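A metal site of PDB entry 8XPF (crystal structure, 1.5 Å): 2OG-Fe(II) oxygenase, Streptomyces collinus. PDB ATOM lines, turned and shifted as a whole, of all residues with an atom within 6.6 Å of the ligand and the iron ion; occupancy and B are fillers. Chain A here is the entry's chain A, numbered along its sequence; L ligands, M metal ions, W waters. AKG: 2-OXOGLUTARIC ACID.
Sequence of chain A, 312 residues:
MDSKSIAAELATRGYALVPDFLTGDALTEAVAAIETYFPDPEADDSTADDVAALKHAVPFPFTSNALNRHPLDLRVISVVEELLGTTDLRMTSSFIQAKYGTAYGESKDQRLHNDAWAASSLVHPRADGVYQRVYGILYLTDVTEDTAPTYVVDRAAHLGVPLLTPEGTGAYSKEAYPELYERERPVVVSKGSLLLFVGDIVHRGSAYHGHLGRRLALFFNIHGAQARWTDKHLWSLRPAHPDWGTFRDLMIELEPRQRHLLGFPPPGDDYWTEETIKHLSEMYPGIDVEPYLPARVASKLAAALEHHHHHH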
ATOM      1  N   PHE A  95       7.617  31.652 -37.303  1.00  0.00           N
ATOM      2  CA  PHE A  95       7.559  30.254 -37.701  1.00  0.00           C
ATOM      3  C   PHE A  95       7.325  29.409 -36.462  1.00  0.00           C
ATOM      4  O   PHE A  95       7.501  29.883 -35.334  1.00  0.00           O
ATOM      5  CB  PHE A  95       8.841  29.801 -38.443  1.00  0.00           C
ATOM      6  CG  PHE A  95      10.102  29.953 -37.628  1.00  0.00           C
ATOM      7  CD1 PHE A  95      10.549  28.897 -36.846  1.00  0.00           C
ATOM      8  CD2 PHE A  95      10.852  31.118 -37.673  1.00  0.00           C
ATOM      9  CE1 PHE A  95      11.736  29.013 -36.103  1.00  0.00           C
ATOM     10  CE2 PHE A  95      12.030  31.250 -36.913  1.00  0.00           C
ATOM     11  CZ  PHE A  95      12.452  30.183 -36.144  1.00  0.00           C
ATOM     12  N   GLN A  97       8.336  25.488 -34.803  1.00  0.00           N
ATOM     13  CA  GLN A  97       9.303  24.419 -34.984  1.00  0.00           C
ATOM     14  C   GLN A  97       9.240  23.463 -33.810  1.00  0.00           C
ATOM     15  O   GLN A  97       8.967  23.861 -32.668  1.00  0.00           O
ATOM     16  CB  GLN A  97      10.734  24.967 -35.126  1.00  0.00           C
ATOM     17  CG  GLN A  97      11.743  23.943 -35.679  1.00  0.00           C
ATOM     18  CD  GLN A  97      13.095  24.564 -35.986  1.00  0.00           C
ATOM     19  OE1 GLN A  97      13.609  25.406 -35.233  1.00  0.00           O
ATOM     20  NE2 GLN A  97      13.709  24.119 -37.091  1.00  0.00           N
ATOM     21  N   LYS A  99      11.659  20.482 -31.934  1.00  0.00           N
ATOM     22  CA  LYS A  99      13.001  19.935 -31.818  1.00  0.00           C
ATOM     23  C   LYS A  99      12.898  18.590 -31.107  1.00  0.00           C
ATOM     24  O   LYS A  99      12.456  18.525 -29.958  1.00  0.00           O
ATOM     25  CB  LYS A  99      13.923  20.873 -31.037  1.00  0.00           C
ATOM     26  CG  LYS A  99      15.358  20.428 -31.077  1.00  0.00           C
ATOM     27  CD  LYS A  99      16.265  21.427 -30.412  1.00  0.00           C
ATOM     28  CE  LYS A  99      16.507  22.626 -31.289  1.00  0.00           C
ATOM     29  NZ  LYS A  99      17.685  23.412 -30.789  1.00  0.00           N
ATOM     30  N   GLN A 110      23.751  24.435 -31.629  1.00  0.00           N
ATOM     31  CA  GLN A 110      24.176  25.538 -32.475  1.00  0.00           C
ATOM     32  C   GLN A 110      25.395  26.211 -31.844  1.00  0.00           C
ATOM     33  O   GLN A 110      25.621  26.135 -30.638  1.00  0.00           O
ATOM     34  CB  GLN A 110      23.079  26.597 -32.547  1.00  0.00           C
ATOM     35  CG  GLN A 110      21.801  26.210 -33.267  1.00  0.00           C
ATOM     36  CD  GLN A 110      20.804  27.378 -33.365  1.00  0.00           C
ATOM     37  OE1 GLN A 110      20.821  28.304 -32.556  1.00  0.00           O
ATOM     38  NE2 GLN A 110      19.932  27.318 -34.364  1.00  0.00           N
ATOM     39  N   HIS A 113      25.829  32.854 -31.253  1.00  0.00           N
ATOM     40  CA  HIS A 113      25.743  33.802 -32.366  1.00  0.00           C
ATOM     41  C   HIS A 113      24.878  34.978 -31.928  1.00  0.00           C
ATOM     42  O   HIS A 113      24.213  34.937 -30.890  1.00  0.00           O
ATOM     43  CB  HIS A 113      25.119  33.128 -33.596  1.00  0.00           C
ATOM     44  CG  HIS A 113      23.702  32.683 -33.391  1.00  0.00           C
ATOM     45  ND1 HIS A 113      23.391  31.447 -32.851  1.00  0.00           N
ATOM     46  CD2 HIS A 113      22.526  33.303 -33.632  1.00  0.00           C
ATOM     47  CE1 HIS A 113      22.075  31.327 -32.786  1.00  0.00           C
ATOM     48  NE2 HIS A 113      21.529  32.442 -33.234  1.00  0.00           N
ATOM     49  N   ASN A 114      24.911  36.036 -32.737  1.00  0.00           N
ATOM     50  CA  ASN A 114      23.926  37.097 -32.636  1.00  0.00           C
ATOM     51  C   ASN A 114      22.987  37.025 -33.838  1.00  0.00           C
ATOM     52  O   ASN A 114      23.295  36.415 -34.859  1.00  0.00           O
ATOM     53  CB  ASN A 114      24.574  38.499 -32.540  1.00  0.00           C
ATOM     54  CG  ASN A 114      25.189  38.965 -33.859  1.00  0.00           C
ATOM     55  OD1 ASN A 114      24.478  39.313 -34.803  1.00  0.00           O
ATOM     56  ND2 ASN A 114      26.512  38.975 -33.932  1.00  0.00           N
ATOM     57  N   ASP A 115      21.812  37.616 -33.646  1.00  0.00           N
ATOM     58  CA  ASP A 115      20.844  37.746 -34.741  1.00  0.00           C
ATOM     59  C   ASP A 115      20.579  39.221 -34.963  1.00  0.00           C
ATOM     60  O   ASP A 115      19.431  39.677 -35.019  1.00  0.00           O
ATOM     61  CB  ASP A 115      19.548  36.995 -34.411  1.00  0.00           C
ATOM     62  CG  ASP A 115      19.680  35.502 -34.563  1.00  0.00           C
ATOM     63  OD1 ASP A 115      19.903  35.027 -35.705  1.00  0.00           O
ATOM     64  OD2 ASP A 115      19.584  34.787 -33.549  1.00  0.00           O
ATOM     65  N   TYR A 135      13.371  39.493 -30.634  1.00  0.00           N
ATOM     66  CA  TYR A 135      13.002  38.105 -30.900  1.00  0.00           C
ATOM     67  C   TYR A 135      12.122  37.583 -29.784  1.00  0.00           C
ATOM     68  O   TYR A 135      12.301  37.949 -28.617  1.00  0.00           O
ATOM     69  CB  TYR A 135      14.260  37.215 -30.972  1.00  0.00           C
ATOM     70  CG  TYR A 135      14.959  37.354 -32.295  1.00  0.00           C
ATOM     71  CD1 TYR A 135      15.629  38.521 -32.623  1.00  0.00           C
ATOM     72  CD2 TYR A 135      14.913  36.325 -33.226  1.00  0.00           C
ATOM     73  CE1 TYR A 135      16.242  38.663 -33.855  1.00  0.00           C
ATOM     74  CE2 TYR A 135      15.532  36.456 -34.451  1.00  0.00           C
ATOM     75  CZ  TYR A 135      16.190  37.627 -34.752  1.00  0.00           C
ATOM     76  OH  TYR A 135      16.780  37.725 -35.981  1.00  0.00           O
ATOM     77  N   GLY A 136      11.176  36.737 -30.138  1.00  0.00           N
ATOM     78  CA  GLY A 136      10.385  36.033 -29.138  1.00  0.00           C
ATOM     79  C   GLY A 136      10.380  34.537 -29.418  1.00  0.00           C
ATOM     80  O   GLY A 136      10.337  34.114 -30.573  1.00  0.00           O
ATOM     81  N   ILE A 137      10.395  33.754 -28.351  1.00  0.00           N
ATOM     82  CA  ILE A 137      10.144  32.323 -28.421  1.00  0.00           C
ATOM     83  C   ILE A 137       9.061  32.022 -27.408  1.00  0.00           C
ATOM     84  O   ILE A 137       9.257  32.199 -26.208  1.00  0.00           O
ATOM     85  CB  ILE A 137      11.395  31.495 -28.120  1.00  0.00           C
ATOM     86  CG1 ILE A 137      12.554  31.945 -29.003  1.00  0.00           C
ATOM     87  CG2 ILE A 137      11.095  30.028 -28.360  1.00  0.00           C
ATOM     88  CD1 ILE A 137      13.864  31.192 -28.738  1.00  0.00           C
ATOM     89  N   TYR A 139       7.178  29.185 -25.741  1.00  0.00           N
ATOM     90  CA  TYR A 139       7.346  27.755 -25.549  1.00  0.00           C
ATOM     91  C   TYR A 139       5.994  27.125 -25.299  1.00  0.00           C
ATOM     92  O   TYR A 139       5.243  27.577 -24.429  1.00  0.00           O
ATOM     93  CB  TYR A 139       8.260  27.496 -24.350  1.00  0.00           C
ATOM     94  CG  TYR A 139       9.630  28.120 -24.500  1.00  0.00           C
ATOM     95  CD1 TYR A 139      10.580  27.552 -25.337  1.00  0.00           C
ATOM     96  CD2 TYR A 139       9.963  29.269 -23.804  1.00  0.00           C
ATOM     97  CE1 TYR A 139      11.859  28.121 -25.468  1.00  0.00           C
ATOM     98  CE2 TYR A 139      11.228  29.833 -23.918  1.00  0.00           C
ATOM     99  CZ  TYR A 139      12.155  29.272 -24.755  1.00  0.00           C
ATOM    100  OH  TYR A 139      13.416  29.851 -24.844  1.00  0.00           O
ATOM    101  N   ALA A 148      16.282  20.781 -24.737  1.00  0.00           N
ATOM    102  CA  ALA A 148      16.821  21.753 -25.692  1.00  0.00           C
ATOM    103  C   ALA A 148      16.522  23.199 -25.292  1.00  0.00           C
ATOM    104  O   ALA A 148      15.935  23.953 -26.079  1.00  0.00           O
ATOM    105  CB  ALA A 148      16.307  21.477 -27.111  1.00  0.00           C
ATOM    106  N   PRO A 149      16.938  23.620 -24.107  1.00  0.00           N
ATOM    107  CA  PRO A 149      16.721  25.017 -23.715  1.00  0.00           C
ATOM    108  C   PRO A 149      17.529  25.973 -24.577  1.00  0.00           C
ATOM    109  O   PRO A 149      18.610  25.634 -25.078  1.00  0.00           O
ATOM    110  CB  PRO A 149      17.227  25.052 -22.271  1.00  0.00           C
ATOM    111  CG  PRO A 149      18.269  23.981 -22.233  1.00  0.00           C
ATOM    112  CD  PRO A 149      17.682  22.881 -23.078  1.00  0.00           C
ATOM    113  N   THR A 150      16.986  27.171 -24.753  1.00  0.00           N
ATOM    114  CA  THR A 150      17.761  28.287 -25.285  1.00  0.00           C
ATOM    115  C   THR A 150      18.862  28.664 -24.296  1.00  0.00           C
ATOM    116  O   THR A 150      18.635  28.684 -23.083  1.00  0.00           O
ATOM    117  CB  THR A 150      16.848  29.490 -25.458  1.00  0.00           C
ATOM    118  OG1 THR A 150      15.685  29.113 -26.214  1.00  0.00           O
ATOM    119  CG2 THR A 150      17.557  30.599 -26.215  1.00  0.00           C
ATOM    120  N   TYR A 151      20.061  28.935 -24.805  1.00  0.00           N
ATOM    121  CA  TYR A 151      21.153  29.466 -23.987  1.00  0.00           C
ATOM    122  C   TYR A 151      21.362  30.936 -24.310  1.00  0.00           C
ATOM    123  O   TYR A 151      21.273  31.349 -25.473  1.00  0.00           O
ATOM    124  CB  TYR A 151      22.461  28.716 -24.224  1.00  0.00           C
ATOM    125  CG  TYR A 151      22.623  27.422 -23.453  1.00  0.00           C
ATOM    126  CD1 TYR A 151      21.902  26.287 -23.821  1.00  0.00           C
ATOM    127  CD2 TYR A 151      23.488  27.343 -22.373  1.00  0.00           C
ATOM    128  CE1 TYR A 151      22.046  25.098 -23.127  1.00  0.00           C
ATOM    129  CE2 TYR A 151      23.630  26.164 -21.677  1.00  0.00           C
ATOM    130  CZ  TYR A 151      22.909  25.053 -22.063  1.00  0.00           C
ATOM    131  OH  TYR A 151      23.076  23.884 -21.354  1.00  0.00           O
ATOM    132  N   LEU A 195      10.040  33.893 -24.041  1.00  0.00           N
ATOM    133  CA  LEU A 195      11.364  34.484 -23.935  1.00  0.00           C
ATOM    134  C   LEU A 195      11.451  35.601 -24.966  1.00  0.00           C
ATOM    135  O   LEU A 195      11.235  35.360 -26.165  1.00  0.00           O
ATOM    136  CB  LEU A 195      12.468  33.456 -24.190  1.00  0.00           C
ATOM    137  CG  LEU A 195      13.882  34.033 -24.168  1.00  0.00           C
ATOM    138  CD1 LEU A 195      14.243  34.499 -22.768  1.00  0.00           C
ATOM    139  CD2 LEU A 195      14.893  32.989 -24.670  1.00  0.00           C
ATOM    140  N   PHE A 197      14.159  38.526 -26.464  1.00  0.00           N
ATOM    141  CA  PHE A 197      15.564  38.899 -26.455  1.00  0.00           C
ATOM    142  C   PHE A 197      15.880  39.858 -27.592  1.00  0.00           C
ATOM    143  O   PHE A 197      15.179  39.912 -28.602  1.00  0.00           O
ATOM    144  CB  PHE A 197      16.513  37.685 -26.419  1.00  0.00           C
ATOM    145  CG  PHE A 197      16.438  36.774 -27.617  1.00  0.00           C
ATOM    146  CD1 PHE A 197      17.269  36.968 -28.715  1.00  0.00           C
ATOM    147  CD2 PHE A 197      15.614  35.657 -27.600  1.00  0.00           C
ATOM    148  CE1 PHE A 197      17.238  36.090 -29.785  1.00  0.00           C
ATOM    149  CE2 PHE A 197      15.569  34.788 -28.674  1.00  0.00           C
ATOM    150  CZ  PHE A 197      16.397  34.988 -29.748  1.00  0.00           C
ATOM    151  N   HIS A 203      23.672  34.151 -28.039  1.00  0.00           N
ATOM    152  CA  HIS A 203      22.757  33.117 -27.601  1.00  0.00           C
ATOM    153  C   HIS A 203      22.879  31.941 -28.568  1.00  0.00           C
ATOM    154  O   HIS A 203      23.517  32.042 -29.619  1.00  0.00           O
ATOM    155  CB  HIS A 203      21.310  33.631 -27.612  1.00  0.00           C
ATOM    156  CG  HIS A 203      20.814  33.894 -28.996  1.00  0.00           C
ATOM    157  ND1 HIS A 203      21.133  35.029 -29.706  1.00  0.00           N
ATOM    158  CD2 HIS A 203      20.065  33.131 -29.836  1.00  0.00           C
ATOM    159  CE1 HIS A 203      20.586  34.974 -30.905  1.00  0.00           C
ATOM    160  NE2 HIS A 203      19.948  33.821 -31.015  1.00  0.00           N
ATOM    161  N   ARG A 204      22.201  30.842 -28.227  1.00  0.00           N
ATOM    162  CA  ARG A 204      22.151  29.706 -29.139  1.00  0.00           C
ATOM    163  C   ARG A 204      21.001  28.795 -28.738  1.00  0.00           C
ATOM    164  O   ARG A 204      20.557  28.792 -27.591  1.00  0.00           O
ATOM    165  CB  ARG A 204      23.451  28.906 -29.117  1.00  0.00           C
ATOM    166  CG  ARG A 204      23.727  28.207 -27.787  1.00  0.00           C
ATOM    167  CD  ARG A 204      25.026  27.403 -27.853  1.00  0.00           C
ATOM    168  NE  ARG A 204      25.345  26.743 -26.590  1.00  0.00           N
ATOM    169  CZ  ARG A 204      24.950  25.511 -26.288  1.00  0.00           C
ATOM    170  NH1 ARG A 204      24.223  24.793 -27.132  1.00  0.00           N
ATOM    171  NH2 ARG A 204      25.293  24.993 -25.115  1.00  0.00           N
ATOM    172  N   GLY A 205      20.538  27.999 -29.703  1.00  0.00           N
ATOM    173  CA  GLY A 205      19.808  26.794 -29.377  1.00  0.00           C
ATOM    174  C   GLY A 205      20.746  25.685 -28.929  1.00  0.00           C
ATOM    175  O   GLY A 205      21.974  25.758 -29.073  1.00  0.00           O
ATOM    176  N   SER A 206      20.162  24.644 -28.346  1.00  0.00           N
ATOM    177  CA  SER A 206      20.952  23.559 -27.789  1.00  0.00           C
ATOM    178  C   SER A 206      20.379  22.213 -28.193  1.00  0.00           C
ATOM    179  O   SER A 206      19.260  22.098 -28.679  1.00  0.00           O
ATOM    180  CB  SER A 206      21.095  23.667 -26.259  1.00  0.00           C
ATOM    181  OG  SER A 206      19.857  23.384 -25.604  1.00  0.00           O
ATOM    182  N   ARG A 215      10.458  19.396 -28.191  1.00  0.00           N
ATOM    183  CA  ARG A 215      10.147  20.752 -27.754  1.00  0.00           C
ATOM    184  C   ARG A 215       9.310  21.427 -28.829  1.00  0.00           C
ATOM    185  O   ARG A 215       9.636  21.341 -30.016  1.00  0.00           O
ATOM    186  CB  ARG A 215      11.429  21.562 -27.535  1.00  0.00           C
ATOM    187  CG  ARG A 215      11.168  22.915 -26.889  1.00  0.00           C
ATOM    188  CD  ARG A 215      12.408  23.819 -26.870  1.00  0.00           C
ATOM    189  NE  ARG A 215      12.667  24.394 -28.178  1.00  0.00           N
ATOM    190  CZ  ARG A 215      13.544  25.364 -28.412  1.00  0.00           C
ATOM    191  NH1 ARG A 215      14.265  25.881 -27.430  1.00  0.00           N
ATOM    192  NH2 ARG A 215      13.681  25.827 -29.641  1.00  0.00           N
ATOM    193  N   PHE A 219       8.075  30.996 -32.874  1.00  0.00           N
ATOM    194  CA  PHE A 219       9.149  31.968 -32.939  1.00  0.00           C
ATOM    195  C   PHE A 219       8.660  33.174 -33.727  1.00  0.00           C
ATOM    196  O   PHE A 219       7.867  33.027 -34.650  1.00  0.00           O
ATOM    197  CB  PHE A 219      10.329  31.397 -33.721  1.00  0.00           C
ATOM    198  CG  PHE A 219      10.980  30.224 -33.062  1.00  0.00           C
ATOM    199  CD1 PHE A 219      10.361  28.985 -33.082  1.00  0.00           C
ATOM    200  CD2 PHE A 219      12.229  30.348 -32.487  1.00  0.00           C
ATOM    201  CE1 PHE A 219      10.970  27.882 -32.495  1.00  0.00           C
ATOM    202  CE2 PHE A 219      12.846  29.257 -31.901  1.00  0.00           C
ATOM    203  CZ  PHE A 219      12.219  28.016 -31.918  1.00  0.00           C
HETATM  204  C1  AKG L   1      16.833  32.074 -32.168  1.00  0.00           C
HETATM  205  O1  AKG L   1      17.281  33.120 -32.649  1.00  0.00           O
HETATM  206  O2  AKG L   1      15.555  31.875 -31.878  1.00  0.00           O
HETATM  207  C2  AKG L   1      17.765  30.864 -31.895  1.00  0.00           C
HETATM  208  O5  AKG L   1      18.974  31.023 -32.019  1.00  0.00           O
HETATM  209  C3  AKG L   1      17.146  29.535 -31.545  1.00  0.00           C
HETATM  210  C4  AKG L   1      17.120  29.261 -30.052  1.00  0.00           C
HETATM  211  C5  AKG L   1      16.299  28.038 -29.691  1.00  0.00           C
HETATM  212  O3  AKG L   1      15.774  27.321 -30.520  1.00  0.00           O
HETATM  213  O4  AKG L   1      16.208  27.828 -28.414  1.00  0.00           O
HETATM  214 FE    FE M   1      19.436  32.926 -32.902  1.00  0.00          FE
HETATM  215  O   HOH W   1      18.909  32.210 -34.824  1.00  0.00           O
HETATM  216  O   HOH W   2      15.818  30.117 -34.668  1.00  0.00           O
HETATM  217  O   HOH W   3      17.243  25.004 -28.373  1.00  0.00           O
HETATM  218  O   HOH W   4      15.166  32.937 -35.154  1.00  0.00           O
HETATM  219  O   HOH W   5      12.846  33.882 -32.138  1.00  0.00           O
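OG1 of Thr 150 lies within hydrogen-bond range of O4 of the ligand (2.6 Å).
The guanidinium group of Arg 215 is in salt-bridge range of an oxygen (O3) of the ligand (2.7 Å).
The side-chain amide oxygen (OE1) of Gln 110 sits close to an oxygen (O5) of the ligand (3.3 Å).
O of Asp 115 lies close to OH of Tyr 135 (3.4 Å).
The side-chain hydroxyl of Thr 150 is in hydrogen-bond range of the side-chain hydroxyl of Tyr 139 (2.8 Å).
O of Lys 99 lies within hydrogen-bond range of N of Arg 215, at 2.8 Å.
The backbone carbonyl oxygen (O) of Ala 148 lies within hydrogen-bond range of the guanidinium group (NH1) of Arg 215 (2.9 Å).
OE1 of Gln 110 lies within hydrogen-bond range of N of Gly 205, at 2.9 Å.
The backbone carbonyl oxygen (O) of Phe 197 is in hydrogen-bond range of the backbone NH (N) of Tyr 135 (2.8 Å).
The backbone carbonyl oxygen (O) of Leu 195 is in hydrogen-bond range of the backbone NH (N) of Ile 137 (2.8 Å).
The backbone NH (N) of Phe 219 lies within hydrogen-bond range of the backbone carbonyl oxygen (O) of Phe 95 (2.8 Å).
Residues that only touch the ligand: Phe 197, Ile 137, Gly 205 and Phe 219.
Hydrophobic or aromatic side chains that line the ligand: His 113, Ile 137, Phe 197, His 203 and Phe 219.
Within 4 Å of the ligand: Gln 110, His 113, Asp 115, Ile 137, Thr 150, Phe 197, His 203, Gly 205, Arg 215 and Phe 219.
Within 4 Å of the iron ion: His 113, Asp 115 and His 203.
The iron ion is bound by the side-chain carboxylate (OD2) of Asp 115 (2.0 Å), water W1 (2.1 Å), an oxygen (O5) of the ligand (2.1 Å), a ring nitrogen (NE2) of His 203 (2.2 Å), a ring nitrogen (NE2) of His 113 (2.2 Å) and an oxygen (O1) of the ligand (2.2 Å).
Water W5 bridges O of Gly 136 and O2 of the ligand.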
